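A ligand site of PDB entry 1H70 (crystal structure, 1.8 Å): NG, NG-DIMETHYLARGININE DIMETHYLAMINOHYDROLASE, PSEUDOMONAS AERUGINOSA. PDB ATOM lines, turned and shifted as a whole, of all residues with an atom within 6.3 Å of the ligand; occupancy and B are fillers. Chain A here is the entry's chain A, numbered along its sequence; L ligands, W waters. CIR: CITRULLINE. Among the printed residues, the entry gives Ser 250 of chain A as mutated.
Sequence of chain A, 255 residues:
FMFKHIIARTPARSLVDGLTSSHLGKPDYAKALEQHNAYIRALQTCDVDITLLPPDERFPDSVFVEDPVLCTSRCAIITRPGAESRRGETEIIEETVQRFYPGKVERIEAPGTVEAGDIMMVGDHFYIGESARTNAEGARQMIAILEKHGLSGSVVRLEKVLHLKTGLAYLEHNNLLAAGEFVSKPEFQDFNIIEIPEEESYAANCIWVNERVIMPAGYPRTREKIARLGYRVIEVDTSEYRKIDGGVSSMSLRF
An oxygen (O7) of the ligand lies within hydrogen-bond range of the side-chain hydroxyl (OG) of Ser 250, 2.5 Å away. The side-chain carboxylate (OD1) of Asp 61 is in salt-bridge range of a nitrogen (N) of the ligand, 2.7 Å away. OD2 of Asp 67 lies within hydrogen-bond range of N6 of the ligand (2.8 Å). N of the ligand lies within hydrogen-bond range of O of Ile 244 (2.8 Å). The backbone carbonyl oxygen of Leu 19 lies within hydrogen-bond range of a nitrogen (N) of the ligand (2.8 Å). The guanidinium group of Arg 133 is in salt-bridge range of an oxygen (O) of the ligand. The guanidinium group (NH1) of Arg 86 lies within salt-bridge range of an oxygen (O) of the ligand (3.0 Å). The side-chain carboxylate (OE1) of Glu 66 is in hydrogen-bond range of a nitrogen (N8) of the ligand, at 3.1 Å.
CD1 of Phe 64 touches C3 of the ligand, 3.7 Å away. Gly 117 touches the ligand. Leu 162 touches the ligand (CD2 to OXT, 3.9 Å). His 163 touches the ligand. Asp 245 touches the ligand (O to C5, 3.4 Å). Hydrophobic or aromatic side chains within 4 Å of the ligand: Leu 19, Phe 64, Leu 162, His 163 and Ile 244. Within 4 Å of the ligand: Leu 19, Asp 61, Phe 64, Glu 66, Asp 67, Arg 86, Gly 117, Arg 133, Leu 162, His 163, Ile 244, Asp 245 and Ser 250. The nearest printed residue that does not touch the ligand is Gly 246 (4.2 Å).
Water W1 lies within hydrogen-bond range of an oxygen (OXT) of the ligand (2.5 Å), the side-chain carboxylate (OD2) of Asp 245 (3.0 Å) and the guanidinium group (NH2) of Arg 133 (3.5 Å). Water W2 lies within hydrogen-bond range of O7 of the ligand (2.6 Å), ND1 of His 163 (2.6 Å) and OG1 of Thr 166 (3.2 Å).
The side-chain carboxylate of Asp 61 sits at hydrogen-bond distance from the backbone NH of Leu 19, 2.8 Å away. NH2 of Arg 86 sits at hydrogen-bond distance from O of Asp 61, 3.3 Å away. The guanidinium group of Arg 86 lies within salt-bridge range of the side-chain carboxylate of Asp 67, at 2.9 Å. NH1 of Arg 133 lies within salt-bridge range of OE1 of Glu 115, 3.0 Å away. The side-chain carboxylate (OE1) of Glu 66 is in hydrogen-bond range of the side-chain hydroxyl (OG) of Ser 249, at 2.7 Å. The backbone carbonyl oxygen (O) of Gly 117 sits at hydrogen-bond distance from the backbone NH (N) of Lys 165, at 3.1 Å. O of His 163 lies close to OG1 of Thr 166. OG of Ser 21 is in hydrogen-bond range of OD2 of Asp 245 (3.0 Å).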
ATOM      1  N   GLY A  18      17.617  11.448 -15.329  1.00  0.00           N
ATOM      2  CA  GLY A  18      18.388  11.250 -16.535  1.00  0.00           C
ATOM      3  C   GLY A  18      19.485  10.209 -16.325  1.00  0.00           C
ATOM      4  O   GLY A  18      19.967  10.043 -15.227  1.00  0.00           O
ATOM      5  N   LEU A  19      19.890   9.553 -17.406  1.00  0.00           N
ATOM      6  CA  LEU A  19      20.955   8.551 -17.313  1.00  0.00           C
ATOM      7  C   LEU A  19      22.262   9.173 -16.842  1.00  0.00           C
ATOM      8  O   LEU A  19      22.548  10.310 -17.192  1.00  0.00           O
ATOM      9  CB  LEU A  19      21.197   7.954 -18.699  1.00  0.00           C
ATOM     10  CG  LEU A  19      20.065   7.169 -19.353  1.00  0.00           C
ATOM     11  CD1 LEU A  19      20.459   6.882 -20.815  1.00  0.00           C
ATOM     12  CD2 LEU A  19      19.792   5.871 -18.582  1.00  0.00           C
ATOM     13  N   THR A  20      23.038   8.451 -16.029  1.00  0.00           N
ATOM     14  CA  THR A  20      24.332   8.964 -15.644  1.00  0.00           C
ATOM     15  C   THR A  20      25.269   7.898 -15.127  1.00  0.00           C
ATOM     16  O   THR A  20      24.857   6.884 -14.578  1.00  0.00           O
ATOM     17  CB  THR A  20      24.228  10.061 -14.581  1.00  0.00           C
ATOM     18  OG1 THR A  20      25.536  10.654 -14.405  1.00  0.00           O
ATOM     19  CG2 THR A  20      23.814   9.503 -13.224  1.00  0.00           C
ATOM     20  N   SER A  21      26.542   8.141 -15.377  1.00  0.00           N
ATOM     21  CA  SER A  21      27.603   7.294 -14.873  1.00  0.00           C
ATOM     22  C   SER A  21      28.426   8.086 -13.837  1.00  0.00           C
ATOM     23  O   SER A  21      29.456   7.604 -13.381  1.00  0.00           O
ATOM     24  CB  SER A  21      28.521   6.875 -16.014  1.00  0.00           C
ATOM     25  OG  SER A  21      29.160   8.010 -16.571  1.00  0.00           O
ATOM     26  N   ASP A  61      16.165  12.519 -20.716  1.00  0.00           N
ATOM     27  CA  ASP A  61      17.373  13.098 -21.323  1.00  0.00           C
ATOM     28  C   ASP A  61      17.102  13.798 -22.652  1.00  0.00           C
ATOM     29  O   ASP A  61      18.054  14.146 -23.365  1.00  0.00           O
ATOM     30  CB  ASP A  61      18.387  11.983 -21.558  1.00  0.00           C
ATOM     31  CG  ASP A  61      19.014  11.452 -20.284  1.00  0.00           C
ATOM     32  OD1 ASP A  61      19.751  12.232 -19.641  1.00  0.00           O
ATOM     33  OD2 ASP A  61      18.798  10.271 -19.910  1.00  0.00           O
ATOM     34  N   PHE A  64      18.956  16.815 -24.323  1.00  0.00           N
ATOM     35  CA  PHE A  64      20.191  16.607 -25.078  1.00  0.00           C
ATOM     36  C   PHE A  64      19.907  16.271 -26.539  1.00  0.00           C
ATOM     37  O   PHE A  64      20.183  15.153 -27.040  1.00  0.00           O
ATOM     38  CB  PHE A  64      21.053  15.514 -24.414  1.00  0.00           C
ATOM     39  CG  PHE A  64      21.399  15.871 -22.986  1.00  0.00           C
ATOM     40  CD1 PHE A  64      21.097  14.995 -21.946  1.00  0.00           C
ATOM     41  CD2 PHE A  64      21.991  17.077 -22.707  1.00  0.00           C
ATOM     42  CE1 PHE A  64      21.404  15.323 -20.641  1.00  0.00           C
ATOM     43  CE2 PHE A  64      22.322  17.427 -21.382  1.00  0.00           C
ATOM     44  CZ  PHE A  64      22.029  16.539 -20.351  1.00  0.00           C
ATOM     45  N   GLU A  66      21.388  17.061 -29.147  1.00  0.00           N
ATOM     46  CA  GLU A  66      22.529  16.731 -29.988  1.00  0.00           C
ATOM     47  C   GLU A  66      22.516  15.254 -30.397  1.00  0.00           C
ATOM     48  O   GLU A  66      22.884  14.956 -31.510  1.00  0.00           O
ATOM     49  CB  GLU A  66      23.845  17.016 -29.257  1.00  0.00           C
ATOM     50  CG  GLU A  66      25.091  16.445 -29.918  1.00  0.00           C
ATOM     51  CD  GLU A  66      26.333  17.244 -29.610  1.00  0.00           C
ATOM     52  OE1 GLU A  66      26.956  16.978 -28.559  1.00  0.00           O
ATOM     53  OE2 GLU A  66      26.707  18.113 -30.401  1.00  0.00           O
ATOM     54  N   ASP A  67      22.102  14.330 -29.533  1.00  0.00           N
ATOM     55  CA  ASP A  67      22.214  12.897 -29.877  1.00  0.00           C
ATOM     56  C   ASP A  67      21.309  12.319 -30.966  1.00  0.00           C
ATOM     57  O   ASP A  67      21.763  11.542 -31.803  1.00  0.00           O
ATOM     58  CB  ASP A  67      22.228  12.075 -28.587  1.00  0.00           C
ATOM     59  CG  ASP A  67      23.372  12.488 -27.714  1.00  0.00           C
ATOM     60  OD1 ASP A  67      24.527  12.560 -28.244  1.00  0.00           O
ATOM     61  OD2 ASP A  67      23.201  12.760 -26.524  1.00  0.00           O
ATOM     62  N   ALA A  83      21.398   4.081 -26.235  1.00  0.00           N
ATOM     63  CA  ALA A  83      20.720   4.000 -24.951  1.00  0.00           C
ATOM     64  C   ALA A  83      19.242   3.663 -25.146  1.00  0.00           C
ATOM     65  O   ALA A  83      18.538   4.452 -25.770  1.00  0.00           O
ATOM     66  CB  ALA A  83      20.852   5.304 -24.205  1.00  0.00           C
ATOM     67  N   ARG A  86      16.531   6.287 -24.723  1.00  0.00           N
ATOM     68  CA  ARG A  86      16.619   7.463 -25.571  1.00  0.00           C
ATOM     69  C   ARG A  86      16.358   7.189 -27.049  1.00  0.00           C
ATOM     70  O   ARG A  86      16.287   8.153 -27.813  1.00  0.00           O
ATOM     71  CB  ARG A  86      18.025   8.089 -25.407  1.00  0.00           C
ATOM     72  CG  ARG A  86      18.362   8.471 -23.965  1.00  0.00           C
ATOM     73  CD  ARG A  86      19.505   9.509 -23.937  1.00  0.00           C
ATOM     74  NE  ARG A  86      19.133  10.695 -24.721  1.00  0.00           N
ATOM     75  CZ  ARG A  86      19.976  11.596 -25.155  1.00  0.00           C
ATOM     76  NH1 ARG A  86      21.253  11.519 -24.822  1.00  0.00           N
ATOM     77  NH2 ARG A  86      19.542  12.599 -25.910  1.00  0.00           N
ATOM     78  N   GLU A 115      24.836   7.970 -31.738  1.00  0.00           N
ATOM     79  CA  GLU A 115      24.398   9.137 -30.958  1.00  0.00           C
ATOM     80  C   GLU A 115      25.341  10.236 -31.425  1.00  0.00           C
ATOM     81  O   GLU A 115      26.559  10.070 -31.318  1.00  0.00           O
ATOM     82  CB  GLU A 115      24.431   8.938 -29.433  1.00  0.00           C
ATOM     83  CG  GLU A 115      23.306   8.020 -28.975  1.00  0.00           C
ATOM     84  CD  GLU A 115      23.328   7.625 -27.514  1.00  0.00           C
ATOM     85  OE1 GLU A 115      24.019   8.303 -26.712  1.00  0.00           O
ATOM     86  OE2 GLU A 115      22.622   6.661 -27.173  1.00  0.00           O
ATOM     87  N   ALA A 116      24.765  11.334 -31.934  1.00  0.00           N
ATOM     88  CA  ALA A 116      25.562  12.402 -32.543  1.00  0.00           C
ATOM     89  C   ALA A 116      26.559  13.139 -31.656  1.00  0.00           C
ATOM     90  O   ALA A 116      27.405  13.883 -32.171  1.00  0.00           O
ATOM     91  CB  ALA A 116      24.678  13.407 -33.322  1.00  0.00           C
ATOM     92  N   GLY A 117      26.527  12.927 -30.352  1.00  0.00           N
ATOM     93  CA  GLY A 117      27.530  13.496 -29.455  1.00  0.00           C
ATOM     94  C   GLY A 117      28.893  12.870 -29.748  1.00  0.00           C
ATOM     95  O   GLY A 117      29.939  13.385 -29.364  1.00  0.00           O
ATOM     96  N   ASP A 118      28.863  11.729 -30.447  1.00  0.00           N
ATOM     97  CA  ASP A 118      30.071  11.017 -30.849  1.00  0.00           C
ATOM     98  C   ASP A 118      30.646  11.581 -32.144  1.00  0.00           C
ATOM     99  O   ASP A 118      31.657  11.092 -32.643  1.00  0.00           O
ATOM    100  CB  ASP A 118      29.773   9.536 -31.074  1.00  0.00           C
ATOM    101  CG  ASP A 118      29.904   8.702 -29.815  1.00  0.00           C
ATOM    102  OD1 ASP A 118      30.953   8.842 -29.123  1.00  0.00           O
ATOM    103  OD2 ASP A 118      29.010   7.864 -29.483  1.00  0.00           O
ATOM    104  N   ARG A 133      27.710   3.933 -27.041  1.00  0.00           N
ATOM    105  CA  ARG A 133      26.477   4.426 -27.644  1.00  0.00           C
ATOM    106  C   ARG A 133      26.479   4.399 -29.187  1.00  0.00           C
ATOM    107  O   ARG A 133      25.428   4.320 -29.826  1.00  0.00           O
ATOM    108  CB  ARG A 133      26.207   5.851 -27.186  1.00  0.00           C
ATOM    109  CG  ARG A 133      26.100   5.997 -25.654  1.00  0.00           C
ATOM    110  CD  ARG A 133      24.844   5.326 -25.100  1.00  0.00           C
ATOM    111  NE  ARG A 133      24.751   5.471 -23.637  1.00  0.00           N
ATOM    112  CZ  ARG A 133      24.326   6.574 -23.076  1.00  0.00           C
ATOM    113  NH1 ARG A 133      23.934   7.610 -23.820  1.00  0.00           N
ATOM    114  NH2 ARG A 133      24.245   6.663 -21.747  1.00  0.00           N
ATOM    115  N   LEU A 162      31.966   8.986 -22.362  1.00  0.00           N
ATOM    116  CA  LEU A 162      30.650   8.587 -22.841  1.00  0.00           C
ATOM    117  C   LEU A 162      30.540   8.779 -24.347  1.00  0.00           C
ATOM    118  O   LEU A 162      30.109   7.895 -25.038  1.00  0.00           O
ATOM    119  CB  LEU A 162      29.559   9.413 -22.137  1.00  0.00           C
ATOM    120  CG  LEU A 162      28.131   9.072 -22.549  1.00  0.00           C
ATOM    121  CD1 LEU A 162      27.773   7.634 -22.165  1.00  0.00           C
ATOM    122  CD2 LEU A 162      27.151  10.084 -21.920  1.00  0.00           C
ATOM    123  N   HIS A 163      30.942   9.936 -24.850  1.00  0.00           N
ATOM    124  CA  HIS A 163      30.896  10.208 -26.281  1.00  0.00           C
ATOM    125  C   HIS A 163      32.200  10.928 -26.624  1.00  0.00           C
ATOM    126  O   HIS A 163      32.810  11.540 -25.757  1.00  0.00           O
ATOM    127  CB  HIS A 163      29.800  11.203 -26.714  1.00  0.00           C
ATOM    128  CG  HIS A 163      28.393  10.744 -26.494  1.00  0.00           C
ATOM    129  ND1 HIS A 163      27.597  11.219 -25.466  1.00  0.00           N
ATOM    130  CD2 HIS A 163      27.631   9.869 -27.183  1.00  0.00           C
ATOM    131  CE1 HIS A 163      26.409  10.633 -25.529  1.00  0.00           C
ATOM    132  NE2 HIS A 163      26.392   9.837 -26.563  1.00  0.00           N
ATOM    133  N   LYS A 165      32.703  13.823 -28.032  1.00  0.00           N
ATOM    134  CA  LYS A 165      32.696  15.243 -27.684  1.00  0.00           C
ATOM    135  C   LYS A 165      32.655  15.577 -26.196  1.00  0.00           C
ATOM    136  O   LYS A 165      32.698  16.751 -25.808  1.00  0.00           O
ATOM    137  CB  LYS A 165      31.676  16.042 -28.496  1.00  0.00           C
ATOM    138  CG  LYS A 165      32.078  16.114 -29.978  1.00  0.00           C
ATOM    139  CD  LYS A 165      31.340  17.221 -30.719  1.00  0.00           C
ATOM    140  CE  LYS A 165      29.829  17.012 -30.715  1.00  0.00           C
ATOM    141  NZ  LYS A 165      29.243  17.758 -31.917  1.00  0.00           N
ATOM    142  N   THR A 166      32.687  14.557 -25.358  1.00  0.00           N
ATOM    143  CA  THR A 166      32.834  14.735 -23.916  1.00  0.00           C
ATOM    144  C   THR A 166      34.218  15.329 -23.681  1.00  0.00           C
ATOM    145  O   THR A 166      34.420  16.113 -22.738  1.00  0.00           O
ATOM    146  CB  THR A 166      32.773  13.380 -23.224  1.00  0.00           C
ATOM    147  OG1 THR A 166      31.422  12.876 -23.250  1.00  0.00           O
ATOM    148  CG2 THR A 166      33.163  13.484 -21.740  1.00  0.00           C
ATOM    149  N   ASN A 205      34.278  20.300 -23.369  1.00  0.00           N
ATOM    150  CA  ASN A 205      33.041  20.370 -24.167  1.00  0.00           C
ATOM    151  C   ASN A 205      32.594  21.838 -24.203  1.00  0.00           C
ATOM    152  O   ASN A 205      32.185  22.378 -23.175  1.00  0.00           O
ATOM    153  CB  ASN A 205      31.978  19.457 -23.539  1.00  0.00           C
ATOM    154  CG  ASN A 205      30.710  19.330 -24.364  1.00  0.00           C
ATOM    155  OD1 ASN A 205      30.303  18.217 -24.741  1.00  0.00           O
ATOM    156  ND2 ASN A 205      30.054  20.420 -24.613  1.00  0.00           N
ATOM    157  N   ILE A 244      24.431  14.746 -15.119  1.00  0.00           N
ATOM    158  CA  ILE A 244      23.962  13.665 -15.988  1.00  0.00           C
ATOM    159  C   ILE A 244      24.778  13.646 -17.284  1.00  0.00           C
ATOM    160  O   ILE A 244      24.248  13.421 -18.373  1.00  0.00           O
ATOM    161  CB  ILE A 244      22.419  13.660 -16.210  1.00  0.00           C
ATOM    162  CG1 ILE A 244      21.925  15.020 -16.718  1.00  0.00           C
ATOM    163  CG2 ILE A 244      21.713  13.241 -14.899  1.00  0.00           C
ATOM    164  CD1 ILE A 244      20.385  15.088 -16.947  1.00  0.00           C
ATOM    165  N   ASP A 245      26.086  13.882 -17.145  1.00  0.00           N
ATOM    166  CA  ASP A 245      27.059  13.751 -18.224  1.00  0.00           C
ATOM    167  C   ASP A 245      26.791  14.532 -19.509  1.00  0.00           C
ATOM    168  O   ASP A 245      27.102  14.033 -20.586  1.00  0.00           O
ATOM    169  CB  ASP A 245      27.195  12.262 -18.617  1.00  0.00           C
ATOM    170  CG  ASP A 245      27.632  11.350 -17.482  1.00  0.00           C
ATOM    171  OD1 ASP A 245      28.304  11.816 -16.539  1.00  0.00           O
ATOM    172  OD2 ASP A 245      27.295  10.134 -17.484  1.00  0.00           O
ATOM    173  N   GLY A 246      26.254  15.745 -19.404  1.00  0.00           N
ATOM    174  CA  GLY A 246      25.980  16.562 -20.581  1.00  0.00           C
ATOM    175  C   GLY A 246      26.524  17.979 -20.384  1.00  0.00           C
ATOM    176  O   GLY A 246      26.718  18.420 -19.251  1.00  0.00           O
ATOM    177  N   GLY A 247      26.698  18.690 -21.496  1.00  0.00           N
ATOM    178  CA  GLY A 247      27.182  20.056 -21.474  1.00  0.00           C
ATOM    179  C   GLY A 247      26.561  20.905 -22.578  1.00  0.00           C
ATOM    180  O   GLY A 247      25.484  20.604 -23.103  1.00  0.00           O
ATOM    181  N   SER A 249      27.554  21.332 -25.771  1.00  0.00           N
ATOM    182  CA  SER A 249      27.392  20.802 -27.139  1.00  0.00           C
ATOM    183  C   SER A 249      26.129  19.944 -27.178  1.00  0.00           C
ATOM    184  O   SER A 249      25.388  19.913 -28.133  1.00  0.00           O
ATOM    185  CB  SER A 249      28.585  19.958 -27.606  1.00  0.00           C
ATOM    186  OG  SER A 249      28.481  18.647 -27.074  1.00  0.00           O
ATOM    187  N   SER A 250      25.890  19.275 -26.068  1.00  0.00           N
ATOM    188  CA  SER A 250      24.776  18.328 -25.908  1.00  0.00           C
ATOM    189  C   SER A 250      23.400  18.915 -26.056  1.00  0.00           C
ATOM    190  O   SER A 250      22.470  18.201 -26.453  1.00  0.00           O
ATOM    191  CB  SER A 250      24.846  17.785 -24.465  1.00  0.00           C
ATOM    192  OG  SER A 250      26.220  17.603 -24.112  1.00  0.00           O
ATOM    193  N   MET A 251      23.261  20.165 -25.669  1.00  0.00           N
ATOM    194  CA  MET A 251      21.978  20.829 -25.583  1.00  0.00           C
ATOM    195  C   MET A 251      21.469  21.529 -26.828  1.00  0.00           C
ATOM    196  O   MET A 251      20.404  22.181 -26.785  1.00  0.00           O
ATOM    197  CB  MET A 251      22.015  21.742 -24.347  1.00  0.00           C
ATOM    198  CG  MET A 251      21.963  20.854 -23.094  1.00  0.00           C
ATOM    199  SD  MET A 251      21.718  21.790 -21.566  1.00  0.00           S
ATOM    200  CE  MET A 251      23.264  22.706 -21.622  1.00  0.00           C
HETATM  201  C   CIR L   1      22.884  10.250 -21.487  1.00  0.00           C
HETATM  202  O   CIR L   1      22.593   9.876 -22.658  1.00  0.00           O
HETATM  203  OXT CIR L   1      23.481   9.434 -20.676  1.00  0.00           O
HETATM  204  CA  CIR L   1      22.626  11.676 -21.065  1.00  0.00           C
HETATM  205  N   CIR L   1      22.383  11.728 -19.611  1.00  0.00           N
HETATM  206  C3  CIR L   1      23.822  12.567 -21.452  1.00  0.00           C
HETATM  207  C4  CIR L   1      23.908  12.687 -22.983  1.00  0.00           C
HETATM  208  C5  CIR L   1      25.113  13.531 -23.353  1.00  0.00           C
HETATM  209  N6  CIR L   1      25.190  13.728 -24.814  1.00  0.00           N
HETATM  210  C7  CIR L   1      26.026  14.554 -25.425  1.00  0.00           C
HETATM  211  O7  CIR L   1      26.844  15.260 -24.815  1.00  0.00           O
HETATM  212  N8  CIR L   1      25.966  14.631 -26.766  1.00  0.00           N
HETATM  213  O   HOH W   1      25.211   8.691 -19.066  1.00  0.00           O
HETATM  214  O   HOH W   2      28.469  13.359 -24.253  1.00  0.00           O
